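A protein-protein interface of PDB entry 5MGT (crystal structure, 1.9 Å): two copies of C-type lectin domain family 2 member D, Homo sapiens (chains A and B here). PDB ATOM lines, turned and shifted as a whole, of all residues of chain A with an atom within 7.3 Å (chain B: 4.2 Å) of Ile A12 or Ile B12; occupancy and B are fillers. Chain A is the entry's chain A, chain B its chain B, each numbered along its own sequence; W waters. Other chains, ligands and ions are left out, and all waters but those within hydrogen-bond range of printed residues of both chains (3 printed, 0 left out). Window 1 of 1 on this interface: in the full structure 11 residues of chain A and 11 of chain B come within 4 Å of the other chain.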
ATOM      1  N   CYS A   7     -10.968   8.920 -33.578  1.00  0.00           N
ATOM      2  CA  CYS A   7     -10.963   8.563 -32.185  1.00  0.00           C
ATOM      3  C   CYS A   7     -10.912   7.068 -32.064  1.00  0.00           C
ATOM      4  O   CYS A   7     -11.452   6.384 -32.940  1.00  0.00           O
ATOM      5  CB  CYS A   7     -12.291   9.036 -31.593  1.00  0.00           C
ATOM      6  SG  CYS A   7     -12.451  10.815 -31.523  1.00  0.00           S
ATOM      7  N   PRO A   8     -10.442   6.549 -30.916  1.00  0.00           N
ATOM      8  CA  PRO A   8     -10.564   5.110 -30.706  1.00  0.00           C
ATOM      9  C   PRO A   8     -11.997   4.590 -30.591  1.00  0.00           C
ATOM     10  O   PRO A   8     -12.938   5.360 -30.341  1.00  0.00           O
ATOM     11  CB  PRO A   8      -9.843   4.875 -29.359  1.00  0.00           C
ATOM     12  CG  PRO A   8      -9.247   6.158 -28.947  1.00  0.00           C
ATOM     13  CD  PRO A   8      -9.935   7.234 -29.717  1.00  0.00           C
ATOM     14  N   GLU A   9     -12.139   3.276 -30.774  1.00  0.00           N
ATOM     15  CA  GLU A   9     -13.399   2.584 -30.605  1.00  0.00           C
ATOM     16  C   GLU A   9     -13.988   2.916 -29.216  1.00  0.00           C
ATOM     17  O   GLU A   9     -13.307   2.868 -28.205  1.00  0.00           O
ATOM     18  CB  GLU A   9     -13.185   1.060 -30.730  1.00  0.00           C
ATOM     19  CG  GLU A   9     -14.355   0.192 -30.317  1.00  0.00           C
ATOM     20  CD  GLU A   9     -15.579   0.291 -31.235  1.00  0.00           C
ATOM     21  OE1 GLU A   9     -16.689  -0.081 -30.760  1.00  0.00           O
ATOM     22  OE2 GLU A   9     -15.455   0.683 -32.430  1.00  0.00           O
ATOM     23  N   SER A  10     -15.253   3.222 -29.186  1.00  0.00           N
ATOM     24  CA  SER A  10     -15.959   3.561 -27.933  1.00  0.00           C
ATOM     25  C   SER A  10     -15.806   5.029 -27.529  1.00  0.00           C
ATOM     26  O   SER A  10     -16.313   5.411 -26.477  1.00  0.00           O
ATOM     27  CB  SER A  10     -15.542   2.694 -26.708  1.00  0.00           C
ATOM     28  OG  SER A  10     -15.470   1.307 -27.006  1.00  0.00           O
ATOM     29  N   TRP A  11     -15.055   5.828 -28.277  1.00  0.00           N
ATOM     30  CA  TRP A  11     -14.925   7.236 -27.964  1.00  0.00           C
ATOM     31  C   TRP A  11     -15.713   8.036 -29.003  1.00  0.00           C
ATOM     32  O   TRP A  11     -15.775   7.648 -30.173  1.00  0.00           O
ATOM     33  CB  TRP A  11     -13.487   7.668 -27.951  1.00  0.00           C
ATOM     34  CG  TRP A  11     -12.588   7.014 -26.862  1.00  0.00           C
ATOM     35  CD1 TRP A  11     -12.364   5.666 -26.660  1.00  0.00           C
ATOM     36  CD2 TRP A  11     -11.823   7.697 -25.893  1.00  0.00           C
ATOM     37  NE1 TRP A  11     -11.521   5.487 -25.574  1.00  0.00           N
ATOM     38  CE2 TRP A  11     -11.132   6.721 -25.127  1.00  0.00           C
ATOM     39  CE3 TRP A  11     -11.620   9.058 -25.599  1.00  0.00           C
ATOM     40  CZ2 TRP A  11     -10.281   7.069 -24.091  1.00  0.00           C
ATOM     41  CZ3 TRP A  11     -10.807   9.397 -24.569  1.00  0.00           C
ATOM     42  CH2 TRP A  11     -10.176   8.409 -23.788  1.00  0.00           C
ATOM     43  N   ILE A  12     -16.242   9.180 -28.585  1.00  0.00           N
ATOM     44  CA  ILE A  12     -17.032  10.043 -29.417  1.00  0.00           C
ATOM     45  C   ILE A  12     -16.242  11.265 -29.793  1.00  0.00           C
ATOM     46  O   ILE A  12     -15.567  11.853 -28.955  1.00  0.00           O
ATOM     47  CB  ILE A  12     -18.278  10.461 -28.661  1.00  0.00           C
ATOM     48  CG1 ILE A  12     -18.981   9.187 -28.096  1.00  0.00           C
ATOM     49  CG2 ILE A  12     -19.188  11.299 -29.546  1.00  0.00           C
ATOM     50  CD1 ILE A  12     -19.471   8.179 -29.146  1.00  0.00           C
ATOM     51  N   GLY A  13     -16.361  11.686 -31.050  1.00  0.00           N
ATOM     52  CA  GLY A  13     -15.691  12.879 -31.517  1.00  0.00           C
ATOM     53  C   GLY A  13     -16.443  14.155 -31.428  1.00  0.00           C
ATOM     54  O   GLY A  13     -17.609  14.197 -31.841  1.00  0.00           O
ATOM     55  N   PHE A  14     -15.819  15.225 -30.892  1.00  0.00           N
ATOM     56  CA  PHE A  14     -16.431  16.526 -30.896  1.00  0.00           C
ATOM     57  C   PHE A  14     -15.366  17.631 -30.900  1.00  0.00           C
ATOM     58  O   PHE A  14     -14.463  17.608 -30.036  1.00  0.00           O
ATOM     59  CB  PHE A  14     -17.372  16.660 -29.700  1.00  0.00           C
ATOM     60  CG  PHE A  14     -18.083  17.946 -29.580  1.00  0.00           C
ATOM     61  CD1 PHE A  14     -19.102  18.283 -30.443  1.00  0.00           C
ATOM     62  CD2 PHE A  14     -17.739  18.829 -28.611  1.00  0.00           C
ATOM     63  CE1 PHE A  14     -19.794  19.496 -30.317  1.00  0.00           C
ATOM     64  CE2 PHE A  14     -18.412  20.048 -28.482  1.00  0.00           C
ATOM     65  CZ  PHE A  14     -19.441  20.373 -29.327  1.00  0.00           C
ATOM     66  N   GLN A  15     -15.506  18.616 -31.808  1.00  0.00           N
ATOM     67  CA  GLN A  15     -14.529  19.757 -31.844  1.00  0.00           C
ATOM     68  C   GLN A  15     -13.061  19.356 -31.685  1.00  0.00           C
ATOM     69  O   GLN A  15     -12.327  19.863 -30.822  1.00  0.00           O
ATOM     70  CB  GLN A  15     -14.925  20.797 -30.785  1.00  0.00           C
ATOM     71  CG  GLN A  15     -16.271  21.420 -31.104  1.00  0.00           C
ATOM     72  CD  GLN A  15     -16.659  22.615 -30.253  1.00  0.00           C
ATOM     73  OE1 GLN A  15     -16.042  22.903 -29.208  1.00  0.00           O
ATOM     74  NE2 GLN A  15     -17.720  23.320 -30.692  1.00  0.00           N
ATOM     75  N   LYS A  17     -11.690  16.815 -30.296  1.00  0.00           N
ATOM     76  CA  LYS A  17     -11.343  15.964 -29.153  1.00  0.00           C
ATOM     77  C   LYS A  17     -12.121  14.629 -29.244  1.00  0.00           C
ATOM     78  O   LYS A  17     -13.042  14.493 -30.068  1.00  0.00           O
ATOM     79  CB  LYS A  17     -11.635  16.739 -27.904  1.00  0.00           C
ATOM     80  CG  LYS A  17     -10.757  17.988 -27.756  1.00  0.00           C
ATOM     81  CD  LYS A  17     -11.041  18.793 -26.504  1.00  0.00           C
ATOM     82  CE  LYS A  17     -12.361  19.550 -26.613  1.00  0.00           C
ATOM     83  NZ  LYS A  17     -12.416  20.586 -27.700  1.00  0.00           N
ATOM     84  N   CYS A  18     -11.689  13.642 -28.473  1.00  0.00           N
ATOM     85  CA  CYS A  18     -12.309  12.335 -28.365  1.00  0.00           C
ATOM     86  C   CYS A  18     -12.729  12.189 -26.911  1.00  0.00           C
ATOM     87  O   CYS A  18     -11.958  12.566 -25.989  1.00  0.00           O
ATOM     88  CB  CYS A  18     -11.319  11.241 -28.741  1.00  0.00           C
ATOM     89  SG  CYS A  18     -10.719  11.433 -30.450  1.00  0.00           S
ATOM     90  N   PHE A  19     -13.982  11.771 -26.712  1.00  0.00           N
ATOM     91  CA  PHE A  19     -14.572  11.668 -25.405  1.00  0.00           C
ATOM     92  C   PHE A  19     -14.943  10.231 -25.051  1.00  0.00           C
ATOM     93  O   PHE A  19     -15.565   9.521 -25.864  1.00  0.00           O
ATOM     94  CB  PHE A  19     -15.788  12.624 -25.299  1.00  0.00           C
ATOM     95  CG  PHE A  19     -15.451  14.062 -25.385  1.00  0.00           C
ATOM     96  CD1 PHE A  19     -15.325  14.709 -26.626  1.00  0.00           C
ATOM     97  CD2 PHE A  19     -15.264  14.807 -24.252  1.00  0.00           C
ATOM     98  CE1 PHE A  19     -15.069  16.051 -26.687  1.00  0.00           C
ATOM     99  CE2 PHE A  19     -14.971  16.139 -24.300  1.00  0.00           C
ATOM    100  CZ  PHE A  19     -14.897  16.791 -25.524  1.00  0.00           C
ATOM    101  N   TYR A  20     -14.617   9.801 -23.819  1.00  0.00           N
ATOM    102  CA  TYR A  20     -14.991   8.472 -23.277  1.00  0.00           C
ATOM    103  C   TYR A  20     -15.962   8.608 -22.157  1.00  0.00           C
ATOM    104  O   TYR A  20     -15.728   9.363 -21.217  1.00  0.00           O
ATOM    105  CB  TYR A  20     -13.710   7.787 -22.698  1.00  0.00           C
ATOM    106  CG  TYR A  20     -13.993   6.452 -22.092  1.00  0.00           C
ATOM    107  CD1 TYR A  20     -14.217   5.350 -22.902  1.00  0.00           C
ATOM    108  CD2 TYR A  20     -14.098   6.300 -20.725  1.00  0.00           C
ATOM    109  CE1 TYR A  20     -14.527   4.126 -22.346  1.00  0.00           C
ATOM    110  CE2 TYR A  20     -14.413   5.085 -20.159  1.00  0.00           C
ATOM    111  CZ  TYR A  20     -14.592   4.011 -20.984  1.00  0.00           C
ATOM    112  OH  TYR A  20     -14.888   2.816 -20.473  1.00  0.00           O
ATOM    113  N   PHE A  21     -17.075   7.921 -22.238  1.00  0.00           N
ATOM    114  CA  PHE A  21     -18.122   7.980 -21.189  1.00  0.00           C
ATOM    115  C   PHE A  21     -18.196   6.620 -20.497  1.00  0.00           C
ATOM    116  O   PHE A  21     -18.538   5.602 -21.148  1.00  0.00           O
ATOM    117  CB  PHE A  21     -19.473   8.287 -21.834  1.00  0.00           C
ATOM    118  CG  PHE A  21     -19.511   9.623 -22.520  1.00  0.00           C
ATOM    119  CD1 PHE A  21     -18.967   9.782 -23.774  1.00  0.00           C
ATOM    120  CD2 PHE A  21     -20.128  10.703 -21.914  1.00  0.00           C
ATOM    121  CE1 PHE A  21     -18.994  11.006 -24.389  1.00  0.00           C
ATOM    122  CE2 PHE A  21     -20.164  11.953 -22.552  1.00  0.00           C
ATOM    123  CZ  PHE A  21     -19.608  12.064 -23.806  1.00  0.00           C
ATOM    124  N   PHE A  53     -22.853  19.347 -25.200  1.00  0.00           N
ATOM    125  CA  PHE A  53     -22.556  18.090 -25.884  1.00  0.00           C
ATOM    126  C   PHE A  53     -22.495  16.957 -24.850  1.00  0.00           C
ATOM    127  O   PHE A  53     -23.052  15.860 -25.044  1.00  0.00           O
ATOM    128  CB  PHE A  53     -21.238  18.249 -26.676  1.00  0.00           C
ATOM    129  CG  PHE A  53     -20.569  16.944 -26.999  1.00  0.00           C
ATOM    130  CD1 PHE A  53     -21.149  16.088 -27.900  1.00  0.00           C
ATOM    131  CD2 PHE A  53     -19.467  16.505 -26.284  1.00  0.00           C
ATOM    132  CE1 PHE A  53     -20.602  14.839 -28.194  1.00  0.00           C
ATOM    133  CE2 PHE A  53     -18.909  15.266 -26.568  1.00  0.00           C
ATOM    134  CZ  PHE A  53     -19.494  14.421 -27.511  1.00  0.00           C
ATOM    135  N   TYR A  57     -24.996  13.528 -24.380  1.00  0.00           N
ATOM    136  CA  TYR A  57     -24.606  12.132 -24.536  1.00  0.00           C
ATOM    137  C   TYR A  57     -24.483  11.308 -23.268  1.00  0.00           C
ATOM    138  O   TYR A  57     -24.486  10.069 -23.300  1.00  0.00           O
ATOM    139  CB  TYR A  57     -23.302  12.055 -25.354  1.00  0.00           C
ATOM    140  CG  TYR A  57     -23.013  10.683 -25.902  1.00  0.00           C
ATOM    141  CD1 TYR A  57     -23.719  10.222 -27.000  1.00  0.00           C
ATOM    142  CD2 TYR A  57     -22.111   9.831 -25.312  1.00  0.00           C
ATOM    143  CE1 TYR A  57     -23.484   8.973 -27.530  1.00  0.00           C
ATOM    144  CE2 TYR A  57     -21.845   8.582 -25.850  1.00  0.00           C
ATOM    145  CZ  TYR A  57     -22.557   8.153 -26.933  1.00  0.00           C
ATOM    146  OH  TYR A  57     -22.351   6.938 -27.503  1.00  0.00           O
ATOM    147  N   CYS A 116     -13.683  10.992 -19.852  1.00  0.00           N
ATOM    148  CA  CYS A 116     -12.343  11.398 -20.240  1.00  0.00           C
ATOM    149  C   CYS A 116     -12.366  12.134 -21.554  1.00  0.00           C
ATOM    150  O   CYS A 116     -13.256  11.877 -22.416  1.00  0.00           O
ATOM    151  CB  CYS A 116     -11.416  10.168 -20.479  1.00  0.00           C
ATOM    152  SG  CYS A 116     -11.309   8.990 -19.151  1.00  0.00           S
ATOM    153  N   LYS A 118      -9.414  13.641 -24.798  1.00  0.00           N
ATOM    154  CA  LYS A 118      -8.040  13.808 -25.323  1.00  0.00           C
ATOM    155  C   LYS A 118      -8.136  14.390 -26.757  1.00  0.00           C
ATOM    156  O   LYS A 118      -9.209  14.344 -27.393  1.00  0.00           O
ATOM    157  CB  LYS A 118      -7.314  12.467 -25.306  1.00  0.00           C
ATOM    158  CG  LYS A 118      -7.849  11.362 -26.219  1.00  0.00           C
ATOM    159  CD  LYS A 118      -6.936  10.144 -26.143  1.00  0.00           C
ATOM    160  CE  LYS A 118      -7.586   8.822 -26.476  1.00  0.00           C
ATOM    161  NZ  LYS A 118      -6.765   7.581 -26.126  1.00  0.00           N
ATOM    162  N   SER B  10     -19.065  21.388 -35.037  1.00  0.00           N
ATOM    163  CA  SER B  10     -20.296  21.075 -34.331  1.00  0.00           C
ATOM    164  C   SER B  10     -20.849  19.689 -34.681  1.00  0.00           C
ATOM    165  O   SER B  10     -21.780  19.256 -33.996  1.00  0.00           O
ATOM    166  CB  SER B  10     -21.396  22.141 -34.486  1.00  0.00           C
ATOM    167  OG  SER B  10     -22.236  21.955 -35.638  1.00  0.00           O
ATOM    168  N   TRP B  11     -20.335  19.011 -35.727  1.00  0.00           N
ATOM    169  CA  TRP B  11     -20.888  17.671 -36.076  1.00  0.00           C
ATOM    170  C   TRP B  11     -20.246  16.681 -35.115  1.00  0.00           C
ATOM    171  O   TRP B  11     -19.133  16.893 -34.634  1.00  0.00           O
ATOM    172  CB  TRP B  11     -20.608  17.326 -37.539  1.00  0.00           C
ATOM    173  CG  TRP B  11     -21.385  18.111 -38.570  1.00  0.00           C
ATOM    174  CD1 TRP B  11     -21.551  19.496 -38.659  1.00  0.00           C
ATOM    175  CD2 TRP B  11     -22.076  17.559 -39.703  1.00  0.00           C
ATOM    176  NE1 TRP B  11     -22.296  19.792 -39.778  1.00  0.00           N
ATOM    177  CE2 TRP B  11     -22.634  18.625 -40.422  1.00  0.00           C
ATOM    178  CE3 TRP B  11     -22.300  16.252 -40.151  1.00  0.00           C
ATOM    179  CZ2 TRP B  11     -23.402  18.425 -41.593  1.00  0.00           C
ATOM    180  CZ3 TRP B  11     -23.033  16.069 -41.329  1.00  0.00           C
ATOM    181  CH2 TRP B  11     -23.588  17.138 -42.009  1.00  0.00           C
ATOM    182  N   ILE B  12     -20.938  15.605 -34.804  1.00  0.00           N
ATOM    183  CA  ILE B  12     -20.502  14.680 -33.835  1.00  0.00           C
ATOM    184  C   ILE B  12     -19.879  13.480 -34.566  1.00  0.00           C
ATOM    185  O   ILE B  12     -20.478  12.928 -35.515  1.00  0.00           O
ATOM    186  CB  ILE B  12     -21.682  14.219 -32.933  1.00  0.00           C
ATOM    187  CG1 ILE B  12     -22.560  15.388 -32.424  1.00  0.00           C
ATOM    188  CG2 ILE B  12     -21.164  13.351 -31.800  1.00  0.00           C
ATOM    189  CD1 ILE B  12     -21.767  16.446 -31.708  1.00  0.00           C
ATOM    190  N   GLY B  13     -18.697  13.054 -34.141  1.00  0.00           N
ATOM    191  CA  GLY B  13     -18.027  11.896 -34.715  1.00  0.00           C
ATOM    192  C   GLY B  13     -18.284  10.577 -34.033  1.00  0.00           C
ATOM    193  O   GLY B  13     -18.136  10.439 -32.823  1.00  0.00           O
ATOM    194  N   PHE B  14     -18.677   9.583 -34.813  1.00  0.00           N
ATOM    195  CA  PHE B  14     -18.852   8.233 -34.335  1.00  0.00           C
ATOM    196  C   PHE B  14     -18.367   7.252 -35.417  1.00  0.00           C
ATOM    197  O   PHE B  14     -18.903   7.280 -36.542  1.00  0.00           O
ATOM    198  CB  PHE B  14     -20.357   7.931 -34.021  1.00  0.00           C
ATOM    199  CG  PHE B  14     -20.594   6.521 -33.521  1.00  0.00           C
ATOM    200  CD1 PHE B  14     -20.200   6.143 -32.249  1.00  0.00           C
ATOM    201  CD2 PHE B  14     -21.192   5.559 -34.347  1.00  0.00           C
ATOM    202  CE1 PHE B  14     -20.414   4.881 -31.792  1.00  0.00           C
ATOM    203  CE2 PHE B  14     -21.397   4.306 -33.895  1.00  0.00           C
ATOM    204  CZ  PHE B  14     -20.979   3.940 -32.608  1.00  0.00           C
ATOM    205  N   LYS B  17     -18.105   8.025 -39.274  1.00  0.00           N
ATOM    206  CA  LYS B  17     -19.096   8.970 -39.777  1.00  0.00           C
ATOM    207  C   LYS B  17     -19.182  10.213 -38.911  1.00  0.00           C
ATOM    208  O   LYS B  17     -18.693  10.229 -37.788  1.00  0.00           O
ATOM    209  CB  LYS B  17     -20.443   8.266 -39.844  1.00  0.00           C
ATOM    210  CG  LYS B  17     -20.588   7.254 -40.987  1.00  0.00           C
ATOM    211  CD  LYS B  17     -21.966   6.568 -40.827  1.00  0.00           C
ATOM    212  CE  LYS B  17     -22.213   5.323 -41.681  1.00  0.00           C
ATOM    213  NZ  LYS B  17     -23.684   5.037 -41.821  1.00  0.00           N
ATOM    214  N   CYS B  18     -19.742  11.259 -39.498  1.00  0.00           N
ATOM    215  CA  CYS B  18     -19.979  12.515 -38.898  1.00  0.00           C
ATOM    216  C   CYS B  18     -21.478  12.793 -38.936  1.00  0.00           C
ATOM    217  O   CYS B  18     -22.085  12.662 -39.969  1.00  0.00           O
ATOM    218  CB  CYS B  18     -19.272  13.607 -39.666  1.00  0.00           C
ATOM    219  SG  CYS B  18     -17.463  13.410 -39.757  1.00  0.00           S
ATOM    220  N   PHE B  19     -22.021  13.328 -37.832  1.00  0.00           N
ATOM    221  CA  PHE B  19     -23.476  13.492 -37.666  1.00  0.00           C
ATOM    222  C   PHE B  19     -23.847  14.870 -37.247  1.00  0.00           C
ATOM    223  O   PHE B  19     -23.171  15.455 -36.383  1.00  0.00           O
ATOM    224  CB  PHE B  19     -23.985  12.454 -36.624  1.00  0.00           C
ATOM    225  CG  PHE B  19     -23.827  11.005 -37.057  1.00  0.00           C
ATOM    226  CD1 PHE B  19     -24.833  10.383 -37.782  1.00  0.00           C
ATOM    227  CD2 PHE B  19     -22.716  10.232 -36.673  1.00  0.00           C
ATOM    228  CE1 PHE B  19     -24.763   9.046 -38.157  1.00  0.00           C
ATOM    229  CE2 PHE B  19     -22.607   8.886 -37.078  1.00  0.00           C
ATOM    230  CZ  PHE B  19     -23.659   8.290 -37.805  1.00  0.00           C
ATOM    231  N   PHE B  53     -26.020   4.750 -30.950  1.00  0.00           N
ATOM    232  CA  PHE B  53     -25.360   6.022 -30.817  1.00  0.00           C
ATOM    233  C   PHE B  53     -26.399   7.138 -31.074  1.00  0.00           C
ATOM    234  O   PHE B  53     -26.461   8.113 -30.314  1.00  0.00           O
ATOM    235  CB  PHE B  53     -24.139   6.175 -31.753  1.00  0.00           C
ATOM    236  CG  PHE B  53     -23.736   7.617 -31.982  1.00  0.00           C
ATOM    237  CD1 PHE B  53     -22.998   8.317 -31.027  1.00  0.00           C
ATOM    238  CD2 PHE B  53     -24.075   8.265 -33.146  1.00  0.00           C
ATOM    239  CE1 PHE B  53     -22.742   9.669 -31.179  1.00  0.00           C
ATOM    240  CE2 PHE B  53     -23.762   9.597 -33.341  1.00  0.00           C
ATOM    241  CZ  PHE B  53     -23.106  10.293 -32.362  1.00  0.00           C
ATOM    242  N   TYR B  57     -27.783  10.069 -28.266  1.00  0.00           N
ATOM    243  CA  TYR B  57     -27.553  11.481 -28.387  1.00  0.00           C
ATOM    244  C   TYR B  57     -28.831  12.278 -28.706  1.00  0.00           C
ATOM    245  O   TYR B  57     -28.855  13.461 -28.432  1.00  0.00           O
ATOM    246  CB  TYR B  57     -26.521  11.797 -29.522  1.00  0.00           C
ATOM    247  CG  TYR B  57     -25.992  13.231 -29.481  1.00  0.00           C
ATOM    248  CD1 TYR B  57     -25.029  13.614 -28.551  1.00  0.00           C
ATOM    249  CD2 TYR B  57     -26.462  14.205 -30.320  1.00  0.00           C
ATOM    250  CE1 TYR B  57     -24.566  14.902 -28.495  1.00  0.00           C
ATOM    251  CE2 TYR B  57     -25.997  15.480 -30.271  1.00  0.00           C
ATOM    252  CZ  TYR B  57     -25.014  15.803 -29.343  1.00  0.00           C
ATOM    253  OH  TYR B  57     -24.494  17.080 -29.288  1.00  0.00           O
HETATM  254  O   HOH W   1     -16.273  15.766 -34.503  1.00  0.00           O
HETATM  255  O   HOH W   2     -24.891  19.697 -27.855  1.00  0.00           O
HETATM  256  O   HOH W   3     -17.305  18.868 -33.974  1.00  0.00           O
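CG2 of Ile A12 touches CG2 of Ile B12 (3.6 Å). Gly B13 touches Ile A12. Ile A12 touches Phe B14. CD1 of Ile A12 touches CD1 of Phe B53 (3.9996 Å). Gly A13 touches Ile B12 (O to CA, 3.5 Å). Phe A14 touches Ile B12 (CD1 to CD1, 3.5 Å). Phe A53 touches Ile B12. Phe A53 touches Tyr B57. CE1 of Tyr A57 touches CD1 of Phe B53, 3.6 Å away. Tyr A57 touches Tyr B57.
Of the 10 printed residues of chain B, 5 touch a printed residue of chain A. Along chain B the printed residues that touch a printed residue of chain A span positions 12 to 57. Hydrophobic or aromatic side chains of chain A that line the printed part of chain B: Ile A12, Phe A14, Phe A53 and Tyr A57. Among the printed residues, 11 pairs touch across the chains. Among the printed residues, no Asp or Glu carboxylate lies within 4 Å of a Lys or Arg side-chain nitrogen of the other chain.
The backbone carbonyl oxygen (O) of Ile A12 lies within hydrogen-bond range of the backbone NH (N) of Phe A19 (2.7 Å). O of Phe B19 lies within hydrogen-bond range of N of Ile B12 (2.7 Å). SG of Cys A18 is disulfide-bonded to SG of Cys A7.
Ile A12 touches Gly B13, and with the chains exchanged Gly A13 touches Ile B12. Ile A12 touches Phe B14, and with the chains exchanged Phe A14 touches Ile B12. Ile A12 touches Phe B53, and with the chains exchanged Phe A53 touches Ile B12. Gly A13 touches its own counterpart, Gly B13. Of the 11 pairs that touch across the chains among the printed residues, 11 have their exchanged pair printed and touching as well.
The backbone carbonyl oxygen (O) of Gly A13 sits at hydrogen-bond distance from the backbone NH (N) of Gly B13, 2.8 Å away.
Printed residues of chain B within 4 Å of Ile A12: Ile B12, Gly B13, Phe B14 and Phe B53. Of the printed residues of chain B, Gly A13 touches Ile B12 (3.5 Å) and Gly B13 (2.8 Å). Of the printed residues of chain B, Phe A53 touches Ile B12 and Tyr B57. Printed residues of chain B within 4 Å of Tyr A57: Phe B53 (3.6 Å) and Tyr B57 (3.95 Å). Ile B12 touches four residues of chain A. Of the printed residues of chain A, Gly B13 touches Ile A12 (3.5 Å) and Gly A13 (2.8 Å). Of the printed residues of chain A, Tyr B57 touches Phe A53 (3.7 Å) and Tyr A57 (3.95 Å). The nearest residue of chain A that does not touch Ile B12 is Tyr A57 (6.3 Å). The nearest printed residue of chain A that does not touch Phe B14 is Gly A13 (4.9 Å).
Water W3 lies within hydrogen-bond range of the backbone carbonyl oxygen of Trp B11, the backbone NH of Gln A15 and the backbone NH of Ser B10. Water W2 bridges OH of Tyr B57 (3.0 Å) and N of Phe A53 (3.4 Å). Water W1 lies within hydrogen-bond range of the backbone carbonyl oxygen (O) of Trp B11 (3.1 Å) and the backbone carbonyl oxygen (O) of Gly A13 (3.4 Å).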
